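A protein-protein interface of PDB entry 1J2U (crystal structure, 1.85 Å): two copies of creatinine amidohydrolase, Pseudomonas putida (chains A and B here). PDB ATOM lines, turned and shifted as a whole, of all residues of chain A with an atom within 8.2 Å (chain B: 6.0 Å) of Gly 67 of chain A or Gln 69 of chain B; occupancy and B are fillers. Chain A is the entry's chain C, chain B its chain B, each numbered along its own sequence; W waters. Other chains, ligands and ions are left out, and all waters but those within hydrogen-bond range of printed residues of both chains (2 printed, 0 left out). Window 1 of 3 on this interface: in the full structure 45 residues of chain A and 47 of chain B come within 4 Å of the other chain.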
ATOM      1  N   PHE A   6       2.760   3.982  -6.962  1.00  0.00           N
ATOM      2  CA  PHE A   6       1.461   4.685  -6.947  1.00  0.00           C
ATOM      3  C   PHE A   6       1.549   6.141  -7.406  1.00  0.00           C
ATOM      4  O   PHE A   6       2.289   6.936  -6.837  1.00  0.00           O
ATOM      5  CB  PHE A   6       0.850   4.620  -5.546  1.00  0.00           C
ATOM      6  CG  PHE A   6       0.423   3.252  -5.144  1.00  0.00           C
ATOM      7  CD1 PHE A   6       1.210   2.489  -4.296  1.00  0.00           C
ATOM      8  CD2 PHE A   6      -0.761   2.714  -5.626  1.00  0.00           C
ATOM      9  CE1 PHE A   6       0.818   1.223  -3.913  1.00  0.00           C
ATOM     10  CE2 PHE A   6      -1.159   1.446  -5.252  1.00  0.00           C
ATOM     11  CZ  PHE A   6      -0.364   0.693  -4.402  1.00  0.00           C
ATOM     12  N   GLY A   8      -0.411   8.539  -6.945  1.00  0.00           N
ATOM     13  CA  GLY A   8      -0.767   9.433  -5.864  1.00  0.00           C
ATOM     14  C   GLY A   8       0.402   9.781  -4.942  1.00  0.00           C
ATOM     15  O   GLY A   8       0.392  10.832  -4.295  1.00  0.00           O
ATOM     16  N   MET A  27      -2.009   1.752 -14.599  1.00  0.00           N
ATOM     17  CA  MET A  27      -2.951   0.742 -14.153  1.00  0.00           C
ATOM     18  C   MET A  27      -4.006   1.378 -13.249  1.00  0.00           C
ATOM     19  O   MET A  27      -3.673   2.188 -12.370  1.00  0.00           O
ATOM     20  CB  MET A  27      -2.199  -0.376 -13.412  1.00  0.00           C
ATOM     21  CG  MET A  27      -1.009  -0.927 -14.242  1.00  0.00           C
ATOM     22  SD  MET A  27       0.084  -2.130 -13.447  1.00  0.00           S
ATOM     23  CE  MET A  27      -1.027  -3.495 -13.180  1.00  0.00           C
ATOM     24  N   LEU A  28      -5.279   1.042 -13.490  1.00  0.00           N
ATOM     25  CA  LEU A  28      -6.381   1.549 -12.681  1.00  0.00           C
ATOM     26  C   LEU A  28      -7.203   0.430 -12.048  1.00  0.00           C
ATOM     27  O   LEU A  28      -7.914  -0.305 -12.761  1.00  0.00           O
ATOM     28  CB  LEU A  28      -7.307   2.405 -13.551  1.00  0.00           C
ATOM     29  CG  LEU A  28      -8.573   2.960 -12.867  1.00  0.00           C
ATOM     30  CD1 LEU A  28      -8.202   3.935 -11.775  1.00  0.00           C
ATOM     31  CD2 LEU A  28      -9.509   3.608 -13.899  1.00  0.00           C
ATOM     32  N   PRO A  29      -7.140   0.290 -10.727  1.00  0.00           N
ATOM     33  CA  PRO A  29      -8.000  -0.672 -10.042  1.00  0.00           C
ATOM     34  C   PRO A  29      -9.443  -0.177 -10.019  1.00  0.00           C
ATOM     35  O   PRO A  29      -9.676   1.002  -9.739  1.00  0.00           O
ATOM     36  CB  PRO A  29      -7.447  -0.702  -8.608  1.00  0.00           C
ATOM     37  CG  PRO A  29      -6.124   0.014  -8.673  1.00  0.00           C
ATOM     38  CD  PRO A  29      -6.246   0.991  -9.790  1.00  0.00           C
ATOM     39  N   VAL A  30     -10.395  -1.057 -10.292  1.00  0.00           N
ATOM     40  CA  VAL A  30     -11.797  -0.666 -10.288  1.00  0.00           C
ATOM     41  C   VAL A  30     -12.539  -1.649  -9.412  1.00  0.00           C
ATOM     42  O   VAL A  30     -12.639  -2.841  -9.729  1.00  0.00           O
ATOM     43  CB  VAL A  30     -12.382  -0.650 -11.702  1.00  0.00           C
ATOM     44  CG1 VAL A  30     -13.801  -0.135 -11.668  1.00  0.00           C
ATOM     45  CG2 VAL A  30     -11.543   0.210 -12.609  1.00  0.00           C
ATOM     46  N   GLY A  31     -13.017  -1.156  -8.278  1.00  0.00           N
ATOM     47  CA  GLY A  31     -13.652  -2.000  -7.293  1.00  0.00           C
ATOM     48  C   GLY A  31     -15.089  -1.690  -6.941  1.00  0.00           C
ATOM     49  O   GLY A  31     -15.912  -1.384  -7.812  1.00  0.00           O
ATOM     50  N   ALA A  32     -15.371  -1.811  -5.642  1.00  0.00           N
ATOM     51  CA  ALA A  32     -16.683  -1.619  -5.080  1.00  0.00           C
ATOM     52  C   ALA A  32     -16.616  -1.634  -3.556  1.00  0.00           C
ATOM     53  O   ALA A  32     -15.644  -2.113  -2.960  1.00  0.00           O
ATOM     54  CB  ALA A  32     -17.609  -2.751  -5.544  1.00  0.00           C
ATOM     55  N   ASP A  45     -13.199  -5.770  -3.004  1.00  0.00           N
ATOM     56  CA  ASP A  45     -13.047  -5.614  -4.441  1.00  0.00           C
ATOM     57  C   ASP A  45     -12.158  -4.442  -4.843  1.00  0.00           C
ATOM     58  O   ASP A  45     -11.814  -4.334  -6.005  1.00  0.00           O
ATOM     59  CB  ASP A  45     -14.384  -5.468  -5.122  1.00  0.00           C
ATOM     60  CG  ASP A  45     -15.208  -6.706  -5.029  1.00  0.00           C
ATOM     61  OD1 ASP A  45     -14.666  -7.787  -4.634  1.00  0.00           O
ATOM     62  OD2 ASP A  45     -16.411  -6.664  -5.315  1.00  0.00           O
ATOM     63  N   VAL A  46     -11.855  -3.549  -3.899  1.00  0.00           N
ATOM     64  CA  VAL A  46     -10.865  -2.503  -4.117  1.00  0.00           C
ATOM     65  C   VAL A  46      -9.500  -3.020  -3.662  1.00  0.00           C
ATOM     66  O   VAL A  46      -8.522  -2.934  -4.388  1.00  0.00           O
ATOM     67  CB  VAL A  46     -11.150  -1.219  -3.272  1.00  0.00           C
ATOM     68  CG1 VAL A  46     -10.002  -0.249  -3.400  1.00  0.00           C
ATOM     69  CG2 VAL A  46     -12.433  -0.577  -3.693  1.00  0.00           C
ATOM     70  N   PRO A  49      -7.642  -5.970  -6.227  1.00  0.00           N
ATOM     71  CA  PRO A  49      -6.977  -5.527  -7.461  1.00  0.00           C
ATOM     72  C   PRO A  49      -5.891  -4.501  -7.193  1.00  0.00           C
ATOM     73  O   PRO A  49      -4.899  -4.485  -7.920  1.00  0.00           O
ATOM     74  CB  PRO A  49      -8.118  -4.929  -8.300  1.00  0.00           C
ATOM     75  CG  PRO A  49      -9.217  -4.666  -7.332  1.00  0.00           C
ATOM     76  CD  PRO A  49      -9.080  -5.639  -6.214  1.00  0.00           C
ATOM     77  N   THR A  50      -6.042  -3.679  -6.158  1.00  0.00           N
ATOM     78  CA  THR A  50      -5.009  -2.697  -5.837  1.00  0.00           C
ATOM     79  C   THR A  50      -3.701  -3.413  -5.477  1.00  0.00           C
ATOM     80  O   THR A  50      -2.626  -3.022  -5.930  1.00  0.00           O
ATOM     81  CB  THR A  50      -5.461  -1.774  -4.694  1.00  0.00           C
ATOM     82  OG1 THR A  50      -6.619  -1.019  -5.100  1.00  0.00           O
ATOM     83  CG2 THR A  50      -4.401  -0.696  -4.397  1.00  0.00           C
ATOM     84  N   CYS A  53      -2.272  -5.026  -8.599  1.00  0.00           N
ATOM     85  CA  CYS A  53      -1.697  -3.976  -9.442  1.00  0.00           C
ATOM     86  C   CYS A  53      -0.345  -3.547  -8.903  1.00  0.00           C
ATOM     87  O   CYS A  53       0.610  -3.337  -9.664  1.00  0.00           O
ATOM     88  CB  CYS A  53      -2.591  -2.739  -9.483  1.00  0.00           C
ATOM     89  SG  CYS A  53      -3.987  -2.781 -10.607  1.00  0.00           S
ATOM     90  N   VAL A  64       0.444   2.931 -10.771  1.00  0.00           N
ATOM     91  CA  VAL A  64      -0.925   2.605 -10.383  1.00  0.00           C
ATOM     92  C   VAL A  64      -1.686   3.851  -9.939  1.00  0.00           C
ATOM     93  O   VAL A  64      -1.238   4.594  -9.048  1.00  0.00           O
ATOM     94  CB  VAL A  64      -0.939   1.582  -9.235  1.00  0.00           C
ATOM     95  CG1 VAL A  64      -2.364   1.091  -8.937  1.00  0.00           C
ATOM     96  CG2 VAL A  64      -0.027   0.385  -9.546  1.00  0.00           C
ATOM     97  N   MET A  65      -2.824   4.083 -10.580  1.00  0.00           N
ATOM     98  CA  MET A  65      -3.688   5.217 -10.266  1.00  0.00           C
ATOM     99  C   MET A  65      -4.544   4.923  -9.052  1.00  0.00           C
ATOM    100  O   MET A  65      -4.766   3.757  -8.703  1.00  0.00           O
ATOM    101  CB  MET A  65      -4.628   5.485 -11.440  1.00  0.00           C
ATOM    102  CG  MET A  65      -3.953   5.935 -12.730  1.00  0.00           C
ATOM    103  SD  MET A  65      -3.336   7.626 -12.675  1.00  0.00           S
ATOM    104  CE  MET A  65      -4.903   8.583 -12.768  1.00  0.00           C
ATOM    105  N   PRO A  66      -5.054   5.972  -8.407  1.00  0.00           N
ATOM    106  CA  PRO A  66      -6.011   5.780  -7.325  1.00  0.00           C
ATOM    107  C   PRO A  66      -7.208   4.943  -7.798  1.00  0.00           C
ATOM    108  O   PRO A  66      -7.744   5.193  -8.880  1.00  0.00           O
ATOM    109  CB  PRO A  66      -6.433   7.209  -6.972  1.00  0.00           C
ATOM    110  CG  PRO A  66      -5.226   8.054  -7.327  1.00  0.00           C
ATOM    111  CD  PRO A  66      -4.704   7.393  -8.608  1.00  0.00           C
ATOM    112  N   GLY A  67      -7.620   3.977  -6.991  1.00  0.00           N
ATOM    113  CA  GLY A  67      -8.655   3.048  -7.388  1.00  0.00           C
ATOM    114  C   GLY A  67     -10.063   3.612  -7.313  1.00  0.00           C
ATOM    115  O   GLY A  67     -10.346   4.538  -6.539  1.00  0.00           O
ATOM    116  N   LEU A  68     -10.951   3.051  -8.123  1.00  0.00           N
ATOM    117  CA  LEU A  68     -12.355   3.407  -8.034  1.00  0.00           C
ATOM    118  C   LEU A  68     -12.913   2.573  -6.882  1.00  0.00           C
ATOM    119  O   LEU A  68     -12.886   1.337  -6.904  1.00  0.00           O
ATOM    120  CB  LEU A  68     -13.073   3.138  -9.355  1.00  0.00           C
ATOM    121  CG  LEU A  68     -12.517   3.826 -10.599  1.00  0.00           C
ATOM    122  CD1 LEU A  68     -13.510   3.741 -11.762  1.00  0.00           C
ATOM    123  CD2 LEU A  68     -12.187   5.283 -10.341  1.00  0.00           C
ATOM    124  N   GLN A  69     -13.390   3.273  -5.864  1.00  0.00           N
ATOM    125  CA  GLN A  69     -13.841   2.703  -4.615  1.00  0.00           C
ATOM    126  C   GLN A  69     -15.293   2.249  -4.634  1.00  0.00           C
ATOM    127  O   GLN A  69     -15.697   1.430  -3.811  1.00  0.00           O
ATOM    128  CB  GLN A  69     -13.717   3.766  -3.522  1.00  0.00           C
ATOM    129  CG  GLN A  69     -12.394   4.550  -3.534  1.00  0.00           C
ATOM    130  CD  GLN A  69     -11.244   3.740  -2.971  1.00  0.00           C
ATOM    131  OE1 GLN A  69     -11.308   3.262  -1.833  1.00  0.00           O
ATOM    132  NE2 GLN A  69     -10.190   3.591  -3.758  1.00  0.00           N
ATOM    133  N   TYR A  70     -16.082   2.839  -5.531  1.00  0.00           N
ATOM    134  CA  TYR A  70     -17.494   2.530  -5.669  1.00  0.00           C
ATOM    135  C   TYR A  70     -17.771   2.016  -7.067  1.00  0.00           C
ATOM    136  O   TYR A  70     -17.323   2.605  -8.033  1.00  0.00           O
ATOM    137  CB  TYR A  70     -18.331   3.778  -5.392  1.00  0.00           C
ATOM    138  CG  TYR A  70     -18.127   4.328  -3.997  1.00  0.00           C
ATOM    139  CD1 TYR A  70     -17.160   5.299  -3.742  1.00  0.00           C
ATOM    140  CD2 TYR A  70     -18.894   3.879  -2.932  1.00  0.00           C
ATOM    141  CE1 TYR A  70     -16.966   5.814  -2.465  1.00  0.00           C
ATOM    142  CE2 TYR A  70     -18.693   4.376  -1.647  1.00  0.00           C
ATOM    143  CZ  TYR A  70     -17.737   5.332  -1.415  1.00  0.00           C
ATOM    144  OH  TYR A  70     -17.575   5.819  -0.134  1.00  0.00           O
ATOM    145  N   THR A  98     -17.022   8.236 -14.976  1.00  0.00           N
ATOM    146  CA  THR A  98     -15.792   8.311 -14.205  1.00  0.00           C
ATOM    147  C   THR A  98     -14.624   7.743 -15.024  1.00  0.00           C
ATOM    148  O   THR A  98     -13.560   8.348 -15.153  1.00  0.00           O
ATOM    149  CB  THR A  98     -15.961   7.556 -12.907  1.00  0.00           C
ATOM    150  OG1 THR A  98     -17.037   8.137 -12.131  1.00  0.00           O
ATOM    151  CG2 THR A  98     -14.730   7.697 -12.050  1.00  0.00           C
ATOM    152  N   ILE A 102     -11.376   9.935 -16.548  1.00  0.00           N
ATOM    153  CA  ILE A 102      -9.999   9.538 -16.243  1.00  0.00           C
ATOM    154  C   ILE A 102      -9.193   9.294 -17.523  1.00  0.00           C
ATOM    155  O   ILE A 102      -8.077   9.791 -17.647  1.00  0.00           O
ATOM    156  CB  ILE A 102      -9.961   8.337 -15.300  1.00  0.00           C
ATOM    157  CG1 ILE A 102     -10.429   8.783 -13.910  1.00  0.00           C
ATOM    158  CG2 ILE A 102      -8.546   7.769 -15.203  1.00  0.00           C
ATOM    159  CD1 ILE A 102     -10.757   7.690 -12.932  1.00  0.00           C
ATOM    160  N   MET A 117      -7.935  -2.904 -14.165  1.00  0.00           N
ATOM    161  CA  MET A 117      -8.042  -4.174 -13.466  1.00  0.00           C
ATOM    162  C   MET A 117      -9.312  -4.186 -12.634  1.00  0.00           C
ATOM    163  O   MET A 117      -9.392  -3.559 -11.570  1.00  0.00           O
ATOM    164  CB  MET A 117      -6.814  -4.406 -12.574  1.00  0.00           C
ATOM    165  CG  MET A 117      -6.748  -5.812 -11.969  1.00  0.00           C
ATOM    166  SD  MET A 117      -5.206  -6.239 -11.135  1.00  0.00           S
ATOM    167  CE  MET A 117      -3.992  -5.809 -12.354  1.00  0.00           C
ATOM    168  N   PRO B  29     -14.876  11.484   3.034  1.00  0.00           N
ATOM    169  CA  PRO B  29     -13.796  12.350   2.551  1.00  0.00           C
ATOM    170  C   PRO B  29     -13.938  12.582   1.046  1.00  0.00           C
ATOM    171  O   PRO B  29     -14.222  11.618   0.330  1.00  0.00           O
ATOM    172  CB  PRO B  29     -12.526  11.547   2.855  1.00  0.00           C
ATOM    173  CG  PRO B  29     -12.945  10.381   3.697  1.00  0.00           C
ATOM    174  CD  PRO B  29     -14.392  10.157   3.443  1.00  0.00           C
ATOM    175  N   GLY B  31     -11.803  14.174  -2.079  1.00  0.00           N
ATOM    176  CA  GLY B  31     -10.531  14.750  -2.469  1.00  0.00           C
ATOM    177  C   GLY B  31     -10.296  15.000  -3.933  1.00  0.00           C
ATOM    178  O   GLY B  31     -11.151  15.504  -4.660  1.00  0.00           O
ATOM    179  N   ALA B  32      -9.074  14.690  -4.343  1.00  0.00           N
ATOM    180  CA  ALA B  32      -8.609  14.924  -5.695  1.00  0.00           C
ATOM    181  C   ALA B  32      -7.223  14.297  -5.909  1.00  0.00           C
ATOM    182  O   ALA B  32      -6.529  13.970  -4.946  1.00  0.00           O
ATOM    183  CB  ALA B  32      -8.513  16.423  -5.952  1.00  0.00           C
ATOM    184  N   LEU B  33      -6.861  14.118  -7.176  1.00  0.00           N
ATOM    185  CA  LEU B  33      -5.501  13.740  -7.601  1.00  0.00           C
ATOM    186  C   LEU B  33      -5.008  14.986  -8.335  1.00  0.00           C
ATOM    187  O   LEU B  33      -5.465  15.324  -9.426  1.00  0.00           O
ATOM    188  CB  LEU B  33      -5.508  12.520  -8.505  1.00  0.00           C
ATOM    189  CG  LEU B  33      -4.122  12.046  -8.972  1.00  0.00           C
ATOM    190  CD1 LEU B  33      -3.292  11.557  -7.795  1.00  0.00           C
ATOM    191  CD2 LEU B  33      -4.258  10.952 -10.013  1.00  0.00           C
ATOM    192  N   VAL B  46      -6.843  13.845  -0.777  1.00  0.00           N
ATOM    193  CA  VAL B  46      -7.542  12.665  -0.247  1.00  0.00           C
ATOM    194  C   VAL B  46      -6.994  12.306   1.128  1.00  0.00           C
ATOM    195  O   VAL B  46      -7.751  12.104   2.081  1.00  0.00           O
ATOM    196  CB  VAL B  46      -7.354  11.418  -1.132  1.00  0.00           C
ATOM    197  CG1 VAL B  46      -7.915  10.173  -0.431  1.00  0.00           C
ATOM    198  CG2 VAL B  46      -8.014  11.619  -2.465  1.00  0.00           C
ATOM    199  N   PRO B  66     -15.281   5.041   2.256  1.00  0.00           N
ATOM    200  CA  PRO B  66     -14.200   5.162   1.278  1.00  0.00           C
ATOM    201  C   PRO B  66     -14.226   6.533   0.605  1.00  0.00           C
ATOM    202  O   PRO B  66     -15.283   7.038   0.194  1.00  0.00           O
ATOM    203  CB  PRO B  66     -14.500   4.029   0.279  1.00  0.00           C
ATOM    204  CG  PRO B  66     -15.272   3.026   1.074  1.00  0.00           C
ATOM    205  CD  PRO B  66     -16.089   3.830   2.038  1.00  0.00           C
ATOM    206  N   GLY B  67     -13.059   7.153   0.491  1.00  0.00           N
ATOM    207  CA  GLY B  67     -12.977   8.507  -0.011  1.00  0.00           C
ATOM    208  C   GLY B  67     -13.118   8.659  -1.515  1.00  0.00           C
ATOM    209  O   GLY B  67     -12.815   7.740  -2.289  1.00  0.00           O
ATOM    210  N   LEU B  68     -13.604   9.823  -1.929  1.00  0.00           N
ATOM    211  CA  LEU B  68     -13.630  10.150  -3.333  1.00  0.00           C
ATOM    212  C   LEU B  68     -12.205  10.592  -3.709  1.00  0.00           C
ATOM    213  O   LEU B  68     -11.673  11.571  -3.165  1.00  0.00           O
ATOM    214  CB  LEU B  68     -14.711  11.187  -3.644  1.00  0.00           C
ATOM    215  CG  LEU B  68     -16.151  10.803  -3.238  1.00  0.00           C
ATOM    216  CD1 LEU B  68     -17.150  11.749  -3.893  1.00  0.00           C
ATOM    217  CD2 LEU B  68     -16.519   9.378  -3.578  1.00  0.00           C
ATOM    218  N   GLN B  69     -11.602   9.833  -4.628  1.00  0.00           N
ATOM    219  CA  GLN B  69     -10.199   9.973  -5.019  1.00  0.00           C
ATOM    220  C   GLN B  69      -9.940  11.022  -6.087  1.00  0.00           C
ATOM    221  O   GLN B  69      -8.821  11.531  -6.194  1.00  0.00           O
ATOM    222  CB  GLN B  69      -9.700   8.623  -5.559  1.00  0.00           C
ATOM    223  CG  GLN B  69     -10.017   7.423  -4.690  1.00  0.00           C
ATOM    224  CD  GLN B  69      -9.209   7.379  -3.399  1.00  0.00           C
ATOM    225  OE1 GLN B  69      -7.979   7.335  -3.433  1.00  0.00           O
ATOM    226  NE2 GLN B  69      -9.898   7.333  -2.274  1.00  0.00           N
ATOM    227  N   TYR B  70     -10.964  11.304  -6.893  1.00  0.00           N
ATOM    228  CA  TYR B  70     -10.881  12.224  -8.007  1.00  0.00           C
ATOM    229  C   TYR B  70     -11.913  13.329  -7.845  1.00  0.00           C
ATOM    230  O   TYR B  70     -13.077  13.057  -7.556  1.00  0.00           O
ATOM    231  CB  TYR B  70     -11.118  11.499  -9.329  1.00  0.00           C
ATOM    232  CG  TYR B  70     -10.128  10.380  -9.616  1.00  0.00           C
ATOM    233  CD1 TYR B  70     -10.357   9.096  -9.177  1.00  0.00           C
ATOM    234  CD2 TYR B  70      -8.965  10.620 -10.339  1.00  0.00           C
ATOM    235  CE1 TYR B  70      -9.455   8.069  -9.443  1.00  0.00           C
ATOM    236  CE2 TYR B  70      -8.073   9.615 -10.618  1.00  0.00           C
ATOM    237  CZ  TYR B  70      -8.310   8.347 -10.169  1.00  0.00           C
ATOM    238  OH  TYR B  70      -7.411   7.343 -10.432  1.00  0.00           O
ATOM    239  N   GLY B  71     -11.466  14.567  -8.027  1.00  0.00           N
ATOM    240  CA  GLY B  71     -12.308  15.743  -7.858  1.00  0.00           C
ATOM    241  C   GLY B  71     -12.429  16.598  -9.097  1.00  0.00           C
ATOM    242  O   GLY B  71     -11.976  16.232 -10.188  1.00  0.00           O
ATOM    243  N   THR B  88      -5.741  14.744 -12.319  1.00  0.00           N
ATOM    244  CA  THR B  88      -6.691  13.933 -13.068  1.00  0.00           C
ATOM    245  C   THR B  88      -8.064  14.252 -12.532  1.00  0.00           C
ATOM    246  O   THR B  88      -8.422  13.798 -11.449  1.00  0.00           O
ATOM    247  CB  THR B  88      -6.366  12.473 -12.828  1.00  0.00           C
ATOM    248  OG1 THR B  88      -5.009  12.215 -13.229  1.00  0.00           O
ATOM    249  CG2 THR B  88      -7.260  11.578 -13.703  1.00  0.00           C
HETATM  250  O   HOH W   1      -6.692   4.879  -4.025  1.00  0.00           O
HETATM  251  O   HOH W   2     -10.879   4.865   0.451  1.00  0.00           O
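Of the 23 printed residues of chain A, 8 touch a printed residue of chain B.
Hydrophobic or aromatic side chains of chain A that line the printed part of chain B: Leu 28, Met 65, Pro 66, Tyr 70 and Ile 102.
Printed residues of chain B that touch a printed residue of chain A: Leu 33, Pro 66, Gly 67, Leu 68, Gln 69, Tyr 70 and Thr 88.
Hydrophobic or aromatic side chains of chain B that line the printed part of chain A: Leu 33, Pro 66, Leu 68 and Tyr 70.
Among the printed residues, 15 pairs touch across the chains.
The backbone NH of Leu 68 of chain B is in hydrogen-bond range of the backbone carbonyl oxygen of Pro 29 of chain B, 3.0 Å away.
The backbone NH (N) of Gly 31 of chain B lies within hydrogen-bond range of the backbone carbonyl oxygen (O) of Leu 68 of chain B (2.8 Å).
N of Leu 33 of chain B lies within hydrogen-bond range of O of Gln 69 of chain B (3.4 Å).
The backbone carbonyl oxygen (O) of Leu 33 of chain B is in hydrogen-bond range of the backbone NH (N) of Thr 88 of chain B (3.0 Å).
NE2 of Gln 69 of chain B lies within hydrogen-bond range of O of Gly 67 of chain B (2.9 Å).
N of Met 117 of chain A sits at hydrogen-bond distance from O of Leu 28 of chain A (3.0 Å).
O of Pro 66 of chain B lies within hydrogen-bond range of OH of Tyr 70 of chain A (2.6 Å).
OH of Tyr 70 of chain B lies within hydrogen-bond range of O of Pro 66 of chain A (2.7 Å).
Thr 50 of chain A touches none of the printed residues of chain B.
Of the printed residues of chain B, Gly 67 of chain A touches Gln 69 (3.4 Å).
Printed residues of chain B within 4 Å of Tyr 70 of chain A: Pro 66 (2.6 Å) and Leu 68 (3.8 Å).
Printed residues of chain B within 4 Å of Ile 102 of chain A: Tyr 70.
Printed residues of chain A within 4 Å of Leu 33 of chain B: Gly 8, Met 65 and Pro 66.
Of the printed residues of chain A, Gly 67 of chain B touches Gln 69 (3.5 Å).
Printed residues of chain A within 4 Å of Gln 69 of chain B: Pro 66, Gly 67 and Gln 69.
Of the printed residues of chain A, Thr 88 of chain B touches Met 65 (3.7 Å).
The nearest residue of chain B that does not touch Gly 67 of chain A is Tyr 70 of chain B (4.7 Å).
The nearest residue of chain A that does not touch Gln 69 of chain B is Leu 68 of chain A (5.6 Å).
The nearest printed residue of chain B that does not touch Gln 69 of chain A is Leu 68 of chain B (5.6 Å).
Pro 66 of chain A touches Tyr 70 of chain B, and with the chains exchanged Tyr 70 of chain A touches Pro 66 of chain B.
Gly 67 of chain A touches Gln 69 of chain B, and with the chains exchanged Gln 69 of chain A touches Gly 67 of chain B.
Gln 69 of chain A touches its own counterpart, Gln 69 of chain B.
Tyr 70 of chain A touches Leu 68 of chain B, but with the chains exchanged Leu 68 of chain A does not touch Tyr 70 of chain B (4.004 Å).
9 positions are printed for both chains.
Of the 15 pairs that touch across the chains among the printed residues, 7 have their exchanged pair printed and touching as well.
Among the printed residues, pairs that only touch across the chains: Gly 8 of chain A with Leu 33 of chain B, Leu 28 of chain A with Tyr 70 of chain B, Met 65 of chain A with Leu 33 of chain B, Met 65 of chain A with Tyr 70 of chain B, Met 65 of chain A with Thr 88 of chain B, Pro 66 of chain A with Leu 33 of chain B, Pro 66 of chain A with Gln 69 of chain B, Gly 67 of chain A with Gln 69 of chain B, Gln 69 of chain A with Pro 66 of chain B, Gln 69 of chain A with Gly 67 of chain B, Gln 69 of chain A with Gln 69 of chain B, Tyr 70 of chain A with Leu 68 of chain B and Ile 102 of chain A with Tyr 70 of chain B.
Water W2 lies within hydrogen-bond range of the side-chain amide oxygen of Gln 69 of chain A (2.8 Å) and the backbone NH of Gly 67 of chain B (3.2 Å).
Water W1 bridges OE1 of Gln 69 of chain B (2.8 Å) and N of Gly 67 of chain A (3.2 Å).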
